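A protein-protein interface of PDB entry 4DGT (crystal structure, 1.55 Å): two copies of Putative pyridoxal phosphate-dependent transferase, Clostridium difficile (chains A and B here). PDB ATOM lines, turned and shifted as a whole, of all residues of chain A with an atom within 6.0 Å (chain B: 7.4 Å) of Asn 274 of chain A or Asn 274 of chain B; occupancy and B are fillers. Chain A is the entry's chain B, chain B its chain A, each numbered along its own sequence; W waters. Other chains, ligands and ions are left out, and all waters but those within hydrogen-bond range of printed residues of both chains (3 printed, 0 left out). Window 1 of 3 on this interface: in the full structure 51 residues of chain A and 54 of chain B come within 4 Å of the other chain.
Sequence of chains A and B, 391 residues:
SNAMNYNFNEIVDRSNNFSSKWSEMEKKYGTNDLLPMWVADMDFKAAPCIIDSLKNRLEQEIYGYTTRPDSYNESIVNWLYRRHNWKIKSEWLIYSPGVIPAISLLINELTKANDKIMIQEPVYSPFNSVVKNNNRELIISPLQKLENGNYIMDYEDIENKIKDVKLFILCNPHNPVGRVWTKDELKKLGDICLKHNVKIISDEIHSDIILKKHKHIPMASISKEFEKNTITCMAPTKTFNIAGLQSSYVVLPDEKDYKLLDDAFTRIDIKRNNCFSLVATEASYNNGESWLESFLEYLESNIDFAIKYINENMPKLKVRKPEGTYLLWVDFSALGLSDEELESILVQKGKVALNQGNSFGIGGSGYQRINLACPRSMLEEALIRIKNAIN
Gly 244 of chain A touches Asn 274 of chain B. CD2 of Leu 245 of chain A touches SG of Cys 275 of chain B (3.7 Å). Phe 276 of chain B touches Leu 245 of chain A. C of Asn 273 of chain B touches NE2 of Gln 246 of chain A, 3.6 Å away. Gln 246 of chain A touches Asn 274 of chain B. Asn 274 of chain A touches Gln 246 of chain B. CD2 of Leu 245 of chain B touches SG of Cys 275 of chain A, at 3.6 Å. Phe 276 of chain A touches Leu 245 of chain B. Phe 276 of chain B touches Phe 276 of chain A (CD2 to CD2, 3.5 Å).
The backbone carbonyl oxygen of Thr 66 of chain B is in hydrogen-bond range of the guanidinium group of Arg 272 of chain B (3.1 Å). The guanidinium group of Arg 68 of chain B sits at hydrogen-bond distance from the side-chain amide oxygen of Asn 273 of chain B (2.8 Å). The backbone carbonyl oxygen of Gln 246 of chain A sits at hydrogen-bond distance from the side-chain hydroxyl of Ser 277 of chain A.
Among the printed residues, no Asp or Glu carboxylate lies within 4 Å of a Lys or Arg side-chain nitrogen of the other chain.
Printed residues of chain B within 4 Å of Asn 273 of chain A: Gln 246 (3.6 Å). Of the printed residues of chain B, Asn 274 of chain A touches Gly 244 (3.1 Å), Gln 246 (3.6 Å) and Asn 274 (3.4 Å). Printed residues of chain B within 4 Å of Cys 275 of chain A: Gly 244 and Leu 245. Printed residues of chain B within 4 Å of Phe 276 of chain A: Leu 245 (3.6 Å) and Phe 276 (3.5 Å). Of the printed residues of chain A, Gly 244 of chain B touches Asn 274 and Cys 275. Printed residues of chain A within 4 Å of Arg 272 of chain B: Gln 246 (3.0 Å). Of chain A, only Gly 244 (3.1 Å), Gln 246 (3.5 Å) and Asn 274 (3.4 Å) come within 4 Å of Asn 274 of chain B. The nearest printed residue of chain A that does not touch Asn 273 of chain B is Gly 244 of chain A (4.8 Å).
Gly 244 of chain A touches Cys 275 of chain B, and with the chains exchanged Cys 275 of chain A touches Gly 244 of chain B. Leu 245 of chain A touches Cys 275 of chain B, and with the chains exchanged Cys 275 of chain A touches Leu 245 of chain B. Gln 246 of chain A touches Arg 272 of chain B, and with the chains exchanged Arg 272 of chain A touches Gln 246 of chain B. Gln 246 of chain A touches Asn 274 of chain B, and with the chains exchanged Asn 274 of chain A touches Gln 246 of chain B.
The backbone NH of Gly 244 of chain A sits close to the backbone carbonyl oxygen of Gly 64 of chain B, 3.3 Å away. The backbone carbonyl oxygen of Gly 244 of chain B lies within hydrogen-bond range of the backbone NH of Cys 275 of chain A, 2.9 Å away. NE2 of Gln 246 of chain B sits at hydrogen-bond distance from O of Arg 272 of chain A, at 3.0 Å. The backbone carbonyl oxygen (O) of Arg 272 of chain B is in hydrogen-bond range of the side-chain amide nitrogen (NE2) of Gln 246 of chain A (3.0 Å). The side-chain amide nitrogen (ND2) of Asn 274 of chain A sits close to the side-chain amide nitrogen (ND2) of Asn 274 of chain B, at 3.4 Å. The backbone carbonyl oxygen (O) of Gly 244 of chain A is in hydrogen-bond range of the backbone NH (N) of Cys 275 of chain B.
Water W3 lies within hydrogen-bond range of the side-chain hydroxyl of Tyr 95 of chain B (2.7 Å), the side-chain amide oxygen of Gln 246 of chain A (2.9 Å) and the backbone carbonyl oxygen of Arg 272 of chain B (3.5 Å). Water W2 lies within hydrogen-bond range of the side-chain hydroxyl of Tyr 95 of chain A (2.8 Å), the side-chain amide oxygen of Gln 246 of chain B (2.9 Å) and the backbone carbonyl oxygen of Arg 272 of chain A (3.4 Å).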
ATOM      1  N   THR A  66      17.958  12.107   6.759  1.00  0.00           N
ATOM      2  CA  THR A  66      18.623  13.130   7.546  1.00  0.00           C
ATOM      3  C   THR A  66      17.719  13.714   8.646  1.00  0.00           C
ATOM      4  O   THR A  66      16.576  14.183   8.329  1.00  0.00           O
ATOM      5  CB  THR A  66      19.117  14.206   6.571  1.00  0.00           C
ATOM      6  OG1 THR A  66      20.121  13.600   5.715  1.00  0.00           O
ATOM      7  CG2 THR A  66      19.740  15.405   7.335  1.00  0.00           C
ATOM      8  N   TYR A  95      10.255  23.683   7.732  1.00  0.00           N
ATOM      9  CA  TYR A  95      11.120  23.480   6.586  1.00  0.00           C
ATOM     10  C   TYR A  95      10.231  23.422   5.349  1.00  0.00           C
ATOM     11  O   TYR A  95       9.198  22.765   5.332  1.00  0.00           O
ATOM     12  CB  TYR A  95      11.858  22.129   6.739  1.00  0.00           C
ATOM     13  CG  TYR A  95      12.417  21.586   5.427  1.00  0.00           C
ATOM     14  CD1 TYR A  95      13.577  22.112   4.869  1.00  0.00           C
ATOM     15  CD2 TYR A  95      11.719  20.618   4.705  1.00  0.00           C
ATOM     16  CE1 TYR A  95      14.048  21.659   3.638  1.00  0.00           C
ATOM     17  CE2 TYR A  95      12.172  20.162   3.474  1.00  0.00           C
ATOM     18  CZ  TYR A  95      13.364  20.714   2.958  1.00  0.00           C
ATOM     19  OH  TYR A  95      13.824  20.266   1.713  1.00  0.00           O
ATOM     20  N   GLY A 244      20.501  25.470  -5.681  1.00  0.00           N
ATOM     21  CA  GLY A 244      20.676  24.076  -6.046  1.00  0.00           C
ATOM     22  C   GLY A 244      20.670  23.104  -4.905  1.00  0.00           C
ATOM     23  O   GLY A 244      20.480  21.885  -5.118  1.00  0.00           O
ATOM     24  N   LEU A 245      20.839  23.613  -3.682  1.00  0.00           N
ATOM     25  CA  LEU A 245      20.741  22.772  -2.483  1.00  0.00           C
ATOM     26  C   LEU A 245      19.348  22.614  -1.971  1.00  0.00           C
ATOM     27  O   LEU A 245      19.095  21.614  -1.281  1.00  0.00           O
ATOM     28  CB  LEU A 245      21.728  23.210  -1.392  1.00  0.00           C
ATOM     29  CG  LEU A 245      23.188  23.381  -1.802  1.00  0.00           C
ATOM     30  CD1 LEU A 245      24.138  23.761  -0.683  1.00  0.00           C
ATOM     31  CD2 LEU A 245      23.787  22.154  -2.510  1.00  0.00           C
ATOM     32  N   GLN A 246      18.455  23.578  -2.238  1.00  0.00           N
ATOM     33  CA  GLN A 246      17.089  23.497  -1.891  1.00  0.00           C
ATOM     34  C   GLN A 246      16.879  23.571  -0.370  1.00  0.00           C
ATOM     35  O   GLN A 246      17.032  22.613   0.364  1.00  0.00           O
ATOM     36  CB  GLN A 246      16.420  22.284  -2.528  1.00  0.00           C
ATOM     37  CG  GLN A 246      16.639  22.219  -4.021  1.00  0.00           C
ATOM     38  CD  GLN A 246      15.819  21.144  -4.685  1.00  0.00           C
ATOM     39  OE1 GLN A 246      15.379  20.153  -4.046  1.00  0.00           O
ATOM     40  NE2 GLN A 246      15.637  21.307  -5.979  1.00  0.00           N
ATOM     41  N   ARG A 272      11.930  16.463   5.341  1.00  0.00           N
ATOM     42  CA  ARG A 272      13.364  16.428   5.683  1.00  0.00           C
ATOM     43  C   ARG A 272      14.166  17.235   4.715  1.00  0.00           C
ATOM     44  O   ARG A 272      13.853  17.285   3.528  1.00  0.00           O
ATOM     45  CB  ARG A 272      13.920  14.999   5.649  1.00  0.00           C
ATOM     46  CG  ARG A 272      13.256  14.050   6.666  1.00  0.00           C
ATOM     47  CD  ARG A 272      13.941  12.658   6.690  1.00  0.00           C
ATOM     48  NE  ARG A 272      13.308  11.807   7.708  1.00  0.00           N
ATOM     49  CZ  ARG A 272      13.449  11.923   9.021  1.00  0.00           C
ATOM     50  NH1 ARG A 272      14.285  12.805   9.571  1.00  0.00           N
ATOM     51  NH2 ARG A 272      12.757  11.119   9.810  1.00  0.00           N
ATOM     52  N   ASN A 273      15.165  17.935   5.246  1.00  0.00           N
ATOM     53  CA  ASN A 273      16.212  18.473   4.404  1.00  0.00           C
ATOM     54  C   ASN A 273      16.938  17.313   3.720  1.00  0.00           C
ATOM     55  O   ASN A 273      17.123  16.243   4.283  1.00  0.00           O
ATOM     56  CB  ASN A 273      17.265  19.261   5.201  1.00  0.00           C
ATOM     57  CG  ASN A 273      16.777  20.575   5.754  1.00  0.00           C
ATOM     58  OD1 ASN A 273      16.067  20.619   6.803  1.00  0.00           O
ATOM     59  ND2 ASN A 273      17.268  21.685   5.136  1.00  0.00           N
ATOM     60  N   ASN A 274      17.434  17.566   2.514  1.00  0.00           N
ATOM     61  CA  ASN A 274      18.482  16.701   2.024  1.00  0.00           C
ATOM     62  C   ASN A 274      19.742  16.900   2.871  1.00  0.00           C
ATOM     63  O   ASN A 274      19.894  17.923   3.514  1.00  0.00           O
ATOM     64  CB  ASN A 274      18.698  16.807   0.499  1.00  0.00           C
ATOM     65  CG  ASN A 274      19.405  18.034   0.076  1.00  0.00           C
ATOM     66  OD1 ASN A 274      20.572  18.177   0.370  1.00  0.00           O
ATOM     67  ND2 ASN A 274      18.716  18.918  -0.647  1.00  0.00           N
ATOM     68  N   CYS A 275      20.677  15.953   2.830  1.00  0.00           N
ATOM     69  CA  CYS A 275      21.840  16.011   3.732  1.00  0.00           C
ATOM     70  C   CYS A 275      22.766  17.198   3.521  1.00  0.00           C
ATOM     71  O   CYS A 275      23.372  17.663   4.472  1.00  0.00           O
ATOM     72  CB  CYS A 275      22.638  14.686   3.786  1.00  0.00           C
ATOM     73  SG  CYS A 275      23.234  14.129   2.161  1.00  0.00           S
ATOM     74  N   PHE A 276      22.882  17.635   2.286  1.00  0.00           N
ATOM     75  CA  PHE A 276      23.723  18.757   1.941  1.00  0.00           C
ATOM     76  C   PHE A 276      23.072  20.098   2.271  1.00  0.00           C
ATOM     77  O   PHE A 276      23.742  21.007   2.812  1.00  0.00           O
ATOM     78  CB  PHE A 276      24.181  18.644   0.511  1.00  0.00           C
ATOM     79  CG  PHE A 276      25.143  17.491   0.306  1.00  0.00           C
ATOM     80  CD1 PHE A 276      26.389  17.482   0.929  1.00  0.00           C
ATOM     81  CD2 PHE A 276      24.806  16.450  -0.481  1.00  0.00           C
ATOM     82  CE1 PHE A 276      27.274  16.421   0.748  1.00  0.00           C
ATOM     83  CE2 PHE A 276      25.670  15.387  -0.683  1.00  0.00           C
ATOM     84  CZ  PHE A 276      26.919  15.389  -0.065  1.00  0.00           C
ATOM     85  N   SER A 277      21.787  20.268   1.986  1.00  0.00           N
ATOM     86  CA  SER A 277      21.030  21.442   2.379  1.00  0.00           C
ATOM     87  C   SER A 277      21.098  21.667   3.894  1.00  0.00           C
ATOM     88  O   SER A 277      21.323  22.811   4.368  1.00  0.00           O
ATOM     89  CB  SER A 277      19.595  21.202   1.905  1.00  0.00           C
ATOM     90  OG  SER A 277      18.709  21.961   2.605  1.00  0.00           O
ATOM     91  N   LEU A 278      21.084  20.580   4.677  1.00  0.00           N
ATOM     92  CA  LEU A 278      21.129  20.677   6.128  1.00  0.00           C
ATOM     93  C   LEU A 278      22.420  21.362   6.622  1.00  0.00           C
ATOM     94  O   LEU A 278      22.415  22.311   7.401  1.00  0.00           O
ATOM     95  CB  LEU A 278      21.049  19.253   6.742  1.00  0.00           C
ATOM     96  CG  LEU A 278      20.822  19.404   8.246  1.00  0.00           C
ATOM     97  CD1 LEU A 278      19.341  19.626   8.598  1.00  0.00           C
ATOM     98  CD2 LEU A 278      21.400  18.195   8.970  1.00  0.00           C
ATOM     99  N   VAL A 279      23.548  20.851   6.169  1.00  0.00           N
ATOM    100  CA  VAL A 279      24.844  21.344   6.651  1.00  0.00           C
ATOM    101  C   VAL A 279      25.154  22.729   6.057  1.00  0.00           C
ATOM    102  O   VAL A 279      25.755  23.605   6.730  1.00  0.00           O
ATOM    103  CB  VAL A 279      26.011  20.355   6.419  1.00  0.00           C
ATOM    104  CG1 VAL A 279      25.750  19.008   7.134  1.00  0.00           C
ATOM    105  CG2 VAL A 279      26.322  20.152   4.901  1.00  0.00           C
ATOM    106  N   LEU B  54      29.644  12.946  -6.529  1.00  0.00           N
ATOM    107  CA  LEU B  54      29.404  14.021  -5.613  1.00  0.00           C
ATOM    108  C   LEU B  54      30.624  14.931  -5.447  1.00  0.00           C
ATOM    109  O   LEU B  54      30.532  16.154  -5.377  1.00  0.00           O
ATOM    110  CB  LEU B  54      28.945  13.486  -4.244  1.00  0.00           C
ATOM    111  CG  LEU B  54      27.643  12.670  -4.179  1.00  0.00           C
ATOM    112  CD1 LEU B  54      27.462  12.018  -2.830  1.00  0.00           C
ATOM    113  CD2 LEU B  54      26.458  13.566  -4.522  1.00  0.00           C
ATOM    114  N   ARG B  57      31.056  17.097  -8.512  1.00  0.00           N
ATOM    115  CA  ARG B  57      30.067  18.176  -8.565  1.00  0.00           C
ATOM    116  C   ARG B  57      30.419  19.234  -7.472  1.00  0.00           C
ATOM    117  O   ARG B  57      30.282  20.433  -7.683  1.00  0.00           O
ATOM    118  CB  ARG B  57      28.636  17.640  -8.328  1.00  0.00           C
ATOM    119  CG  ARG B  57      27.569  18.733  -8.362  1.00  0.00           C
ATOM    120  CD  ARG B  57      27.572  19.487  -9.679  1.00  0.00           C
ATOM    121  NE  ARG B  57      26.585  20.583  -9.680  1.00  0.00           N
ATOM    122  CZ  ARG B  57      26.831  21.753  -9.161  1.00  0.00           C
ATOM    123  NH1 ARG B  57      27.945  21.995  -8.499  1.00  0.00           N
ATOM    124  NH2 ARG B  57      25.909  22.694  -9.261  1.00  0.00           N
ATOM    125  N   GLY B  64      23.944  26.599  -7.830  1.00  0.00           N
ATOM    126  CA  GLY B  64      22.730  27.302  -8.273  1.00  0.00           C
ATOM    127  C   GLY B  64      21.653  26.356  -8.761  1.00  0.00           C
ATOM    128  O   GLY B  64      21.768  25.149  -8.679  1.00  0.00           O
ATOM    129  N   THR B  66      19.557  23.939 -10.954  1.00  0.00           N
ATOM    130  CA  THR B  66      20.119  22.805 -11.746  1.00  0.00           C
ATOM    131  C   THR B  66      19.208  22.398 -12.876  1.00  0.00           C
ATOM    132  O   THR B  66      18.005  22.147 -12.633  1.00  0.00           O
ATOM    133  CB  THR B  66      20.173  21.571 -10.922  1.00  0.00           C
ATOM    134  OG1 THR B  66      20.531  21.910  -9.572  1.00  0.00           O
ATOM    135  CG2 THR B  66      21.469  20.868 -11.319  1.00  0.00           C
ATOM    136  N   THR B  67      19.770  22.310 -14.071  1.00  0.00           N
ATOM    137  CA  THR B  67      19.038  21.809 -15.228  1.00  0.00           C
ATOM    138  C   THR B  67      19.208  20.292 -15.236  1.00  0.00           C
ATOM    139  O   THR B  67      20.185  19.777 -14.716  1.00  0.00           O
ATOM    140  CB  THR B  67      19.578  22.449 -16.510  1.00  0.00           C
ATOM    141  OG1 THR B  67      18.656  22.210 -17.581  1.00  0.00           O
ATOM    142  CG2 THR B  67      20.889  21.910 -16.881  1.00  0.00           C
ATOM    143  N   ARG B  68      18.241  19.581 -15.770  1.00  0.00           N
ATOM    144  CA  ARG B  68      18.283  18.138 -15.864  1.00  0.00           C
ATOM    145  C   ARG B  68      18.757  17.800 -17.269  1.00  0.00           C
ATOM    146  O   ARG B  68      18.003  17.980 -18.239  1.00  0.00           O
ATOM    147  CB  ARG B  68      16.900  17.571 -15.607  1.00  0.00           C
ATOM    148  CG  ARG B  68      16.825  16.033 -15.617  1.00  0.00           C
ATOM    149  CD  ARG B  68      15.455  15.501 -15.198  1.00  0.00           C
ATOM    150  NE  ARG B  68      15.111  15.962 -13.867  1.00  0.00           N
ATOM    151  CZ  ARG B  68      14.234  16.902 -13.571  1.00  0.00           C
ATOM    152  NH1 ARG B  68      13.454  17.478 -14.500  1.00  0.00           N
ATOM    153  NH2 ARG B  68      14.124  17.297 -12.329  1.00  0.00           N
ATOM    154  N   TYR B  72      20.503  12.205 -17.707  1.00  0.00           N
ATOM    155  CA  TYR B  72      19.860  11.793 -16.468  1.00  0.00           C
ATOM    156  C   TYR B  72      18.734  10.834 -16.781  1.00  0.00           C
ATOM    157  O   TYR B  72      18.795   9.667 -16.369  1.00  0.00           O
ATOM    158  CB  TYR B  72      19.415  13.057 -15.716  1.00  0.00           C
ATOM    159  CG  TYR B  72      18.608  12.806 -14.440  1.00  0.00           C
ATOM    160  CD1 TYR B  72      19.205  12.802 -13.171  1.00  0.00           C
ATOM    161  CD2 TYR B  72      17.252  12.569 -14.484  1.00  0.00           C
ATOM    162  CE1 TYR B  72      18.487  12.597 -12.030  1.00  0.00           C
ATOM    163  CE2 TYR B  72      16.511  12.329 -13.327  1.00  0.00           C
ATOM    164  CZ  TYR B  72      17.152  12.336 -12.069  1.00  0.00           C
ATOM    165  OH  TYR B  72      16.401  12.140 -10.911  1.00  0.00           O
ATOM    166  N   TYR B  95      10.134  13.778 -12.603  1.00  0.00           N
ATOM    167  CA  TYR B  95      10.863  13.877 -11.332  1.00  0.00           C
ATOM    168  C   TYR B  95       9.968  14.117 -10.147  1.00  0.00           C
ATOM    169  O   TYR B  95       9.012  14.879 -10.204  1.00  0.00           O
ATOM    170  CB  TYR B  95      11.879  15.034 -11.442  1.00  0.00           C
ATOM    171  CG  TYR B  95      12.404  15.454 -10.080  1.00  0.00           C
ATOM    172  CD1 TYR B  95      13.390  14.754  -9.456  1.00  0.00           C
ATOM    173  CD2 TYR B  95      11.870  16.579  -9.435  1.00  0.00           C
ATOM    174  CE1 TYR B  95      13.868  15.152  -8.209  1.00  0.00           C
ATOM    175  CE2 TYR B  95      12.324  16.968  -8.192  1.00  0.00           C
ATOM    176  CZ  TYR B  95      13.346  16.264  -7.594  1.00  0.00           C
ATOM    177  OH  TYR B  95      13.756  16.632  -6.308  1.00  0.00           O
ATOM    178  N   ALA B 243      18.847   7.993   0.131  1.00  0.00           N
ATOM    179  CA  ALA B 243      17.615   8.745   0.513  1.00  0.00           C
ATOM    180  C   ALA B 243      17.857  10.140   0.941  1.00  0.00           C
ATOM    181  O   ALA B 243      16.974  11.018   0.676  1.00  0.00           O
ATOM    182  CB  ALA B 243      16.816   7.938   1.559  1.00  0.00           C
ATOM    183  N   GLY B 244      19.019  10.393   1.543  1.00  0.00           N
ATOM    184  CA  GLY B 244      19.369  11.744   1.971  1.00  0.00           C
ATOM    185  C   GLY B 244      19.583  12.669   0.816  1.00  0.00           C
ATOM    186  O   GLY B 244      19.658  13.903   1.006  1.00  0.00           O
ATOM    187  N   LEU B 245      19.773  12.125  -0.389  1.00  0.00           N
ATOM    188  CA  LEU B 245      19.925  13.014  -1.568  1.00  0.00           C
ATOM    189  C   LEU B 245      18.651  13.382  -2.221  1.00  0.00           C
ATOM    190  O   LEU B 245      18.608  14.398  -2.941  1.00  0.00           O
ATOM    191  CB  LEU B 245      20.874  12.419  -2.597  1.00  0.00           C
ATOM    192  CG  LEU B 245      22.236  11.949  -2.080  1.00  0.00           C
ATOM    193  CD1 LEU B 245      23.144  11.468  -3.222  1.00  0.00           C
ATOM    194  CD2 LEU B 245      22.965  13.050  -1.294  1.00  0.00           C
ATOM    195  N   GLN B 246      17.590  12.593  -1.998  1.00  0.00           N
ATOM    196  CA  GLN B 246      16.226  12.869  -2.438  1.00  0.00           C
ATOM    197  C   GLN B 246      16.105  12.828  -3.970  1.00  0.00           C
ATOM    198  O   GLN B 246      16.405  13.783  -4.703  1.00  0.00           O
ATOM    199  CB  GLN B 246      15.704  14.199  -1.881  1.00  0.00           C
ATOM    200  CG  GLN B 246      15.780  14.195  -0.385  1.00  0.00           C
ATOM    201  CD  GLN B 246      15.135  15.415   0.255  1.00  0.00           C
ATOM    202  OE1 GLN B 246      14.970  16.453  -0.379  1.00  0.00           O
ATOM    203  NE2 GLN B 246      14.847  15.314   1.526  1.00  0.00           N
ATOM    204  N   SER B 247      15.673  11.714  -4.463  1.00  0.00           N
ATOM    205  CA  SER B 247      15.504  11.598  -5.910  1.00  0.00           C
ATOM    206  C   SER B 247      14.589  10.455  -6.149  1.00  0.00           C
ATOM    207  O   SER B 247      14.798   9.401  -5.615  1.00  0.00           O
ATOM    208  CB  SER B 247      16.867  11.252  -6.555  1.00  0.00           C
ATOM    209  OG  SER B 247      16.731  10.876  -7.910  1.00  0.00           O
ATOM    210  N   LYS B 271      10.071  20.925  -9.275  1.00  0.00           N
ATOM    211  CA  LYS B 271      10.425  20.560 -10.621  1.00  0.00           C
ATOM    212  C   LYS B 271      11.861  20.112 -10.793  1.00  0.00           C
ATOM    213  O   LYS B 271      12.169  19.298 -11.660  1.00  0.00           O
ATOM    214  CB  LYS B 271      10.199  21.735 -11.596  1.00  0.00           C
ATOM    215  CG  LYS B 271       8.769  22.303 -11.638  1.00  0.00           C
ATOM    216  CD  LYS B 271       7.693  21.327 -12.066  1.00  0.00           C
ATOM    217  CE  LYS B 271       7.527  21.187 -13.515  1.00  0.00           C
ATOM    218  NZ  LYS B 271       6.230  20.534 -13.864  1.00  0.00           N
ATOM    219  N   ARG B 272      12.771  20.645 -10.013  1.00  0.00           N
ATOM    220  CA  ARG B 272      14.185  20.438 -10.236  1.00  0.00           C
ATOM    221  C   ARG B 272      14.766  19.457  -9.233  1.00  0.00           C
ATOM    222  O   ARG B 272      14.438  19.524  -8.045  1.00  0.00           O
ATOM    223  CB  ARG B 272      14.954  21.769 -10.124  1.00  0.00           C
ATOM    224  CG  ARG B 272      14.569  22.786 -11.179  1.00  0.00           C
ATOM    225  CD  ARG B 272      15.515  24.007 -11.165  1.00  0.00           C
ATOM    226  NE  ARG B 272      15.076  25.016 -12.147  1.00  0.00           N
ATOM    227  CZ  ARG B 272      15.253  24.925 -13.465  1.00  0.00           C
ATOM    228  NH1 ARG B 272      15.956  23.928 -14.042  1.00  0.00           N
ATOM    229  NH2 ARG B 272      14.746  25.885 -14.241  1.00  0.00           N
ATOM    230  N   ASN B 273      15.744  18.682  -9.663  1.00  0.00           N
ATOM    231  CA  ASN B 273      16.564  17.910  -8.695  1.00  0.00           C
ATOM    232  C   ASN B 273      17.455  18.907  -7.996  1.00  0.00           C
ATOM    233  O   ASN B 273      17.863  19.904  -8.661  1.00  0.00           O
ATOM    234  CB  ASN B 273      17.531  16.974  -9.427  1.00  0.00           C
ATOM    235  CG  ASN B 273      16.902  15.761 -10.030  1.00  0.00           C
ATOM    236  OD1 ASN B 273      16.203  15.850 -11.098  1.00  0.00           O
ATOM    237  ND2 ASN B 273      17.192  14.598  -9.420  1.00  0.00           N
ATOM    238  N   ASN B 274      17.832  18.636  -6.749  1.00  0.00           N
ATOM    239  CA  ASN B 274      18.964  19.307  -6.194  1.00  0.00           C
ATOM    240  C   ASN B 274      20.248  18.869  -6.910  1.00  0.00           C
ATOM    241  O   ASN B 274      20.285  17.891  -7.630  1.00  0.00           O
ATOM    242  CB  ASN B 274      19.014  19.177  -4.675  1.00  0.00           C
ATOM    243  CG  ASN B 274      19.522  17.840  -4.203  1.00  0.00           C
ATOM    244  OD1 ASN B 274      20.670  17.507  -4.481  1.00  0.00           O
ATOM    245  ND2 ASN B 274      18.678  17.073  -3.492  1.00  0.00           N
ATOM    246  N   CYS B 275      21.292  19.684  -6.806  1.00  0.00           N
ATOM    247  CA  CYS B 275      22.436  19.472  -7.677  1.00  0.00           C
ATOM    248  C   CYS B 275      23.177  18.164  -7.451  1.00  0.00           C
ATOM    249  O   CYS B 275      23.731  17.578  -8.389  1.00  0.00           O
ATOM    250  CB  CYS B 275      23.407  20.657  -7.656  1.00  0.00           C
ATOM    251  SG  CYS B 275      24.081  21.058  -6.054  1.00  0.00           S
ATOM    252  N   PHE B 276      23.129  17.688  -6.223  1.00  0.00           N
ATOM    253  CA  PHE B 276      23.788  16.417  -5.866  1.00  0.00           C
ATOM    254  C   PHE B 276      22.973  15.180  -6.250  1.00  0.00           C
ATOM    255  O   PHE B 276      23.480  14.171  -6.675  1.00  0.00           O
ATOM    256  CB  PHE B 276      24.177  16.439  -4.378  1.00  0.00           C
ATOM    257  CG  PHE B 276      25.308  17.406  -4.076  1.00  0.00           C
ATOM    258  CD1 PHE B 276      26.570  17.234  -4.678  1.00  0.00           C
ATOM    259  CD2 PHE B 276      25.112  18.522  -3.296  1.00  0.00           C
ATOM    260  CE1 PHE B 276      27.603  18.137  -4.414  1.00  0.00           C
ATOM    261  CE2 PHE B 276      26.142  19.411  -3.044  1.00  0.00           C
ATOM    262  CZ  PHE B 276      27.399  19.214  -3.629  1.00  0.00           C
ATOM    263  N   SER B 277      21.675  15.228  -6.015  1.00  0.00           N
ATOM    264  CA  SER B 277      20.766  14.240  -6.494  1.00  0.00           C
ATOM    265  C   SER B 277      20.914  13.992  -7.971  1.00  0.00           C
ATOM    266  O   SER B 277      20.879  12.861  -8.443  1.00  0.00           O
ATOM    267  CB  SER B 277      19.343  14.775  -6.251  1.00  0.00           C
ATOM    268  OG  SER B 277      18.367  14.010  -6.857  1.00  0.00           O
ATOM    269  N   LEU B 278      21.080  15.088  -8.734  1.00  0.00           N
ATOM    270  CA  LEU B 278      21.188  14.991 -10.177  1.00  0.00           C
ATOM    271  C   LEU B 278      22.357  14.070 -10.570  1.00  0.00           C
ATOM    272  O   LEU B 278      22.189  13.111 -11.314  1.00  0.00           O
ATOM    273  CB  LEU B 278      21.379  16.373 -10.813  1.00  0.00           C
ATOM    274  CG  LEU B 278      21.231  16.292 -12.319  1.00  0.00           C
ATOM    275  CD1 LEU B 278      19.711  16.378 -12.649  1.00  0.00           C
ATOM    276  CD2 LEU B 278      22.062  17.286 -13.094  1.00  0.00           C
ATOM    277  N   VAL B 279      23.533  14.347 -10.044  1.00  0.00           N
ATOM    278  CA  VAL B 279      24.702  13.618 -10.464  1.00  0.00           C
ATOM    279  C   VAL B 279      24.763  12.213  -9.863  1.00  0.00           C
ATOM    280  O   VAL B 279      25.238  11.263 -10.487  1.00  0.00           O
ATOM    281  CB  VAL B 279      25.973  14.435 -10.202  1.00  0.00           C
ATOM    282  CG1 VAL B 279      25.876  15.807 -10.907  1.00  0.00           C
ATOM    283  CG2 VAL B 279      26.320  14.570  -8.707  1.00  0.00           C
ATOM    284  N   ALA B 280      24.227  12.048  -8.665  1.00  0.00           N
ATOM    285  CA  ALA B 280      24.326  10.764  -7.966  1.00  0.00           C
ATOM    286  C   ALA B 280      23.373   9.767  -8.570  1.00  0.00           C
ATOM    287  O   ALA B 280      23.648   8.586  -8.616  1.00  0.00           O
ATOM    288  CB  ALA B 280      24.004  10.922  -6.473  1.00  0.00           C
HETATM  289  O   HOH W   1      16.276  18.135  -2.184  1.00  0.00           O
HETATM  290  O   HOH W   2      12.711  18.076   0.425  1.00  0.00           O
HETATM  291  O   HOH W   3      12.989  18.846  -4.952  1.00  0.00           O
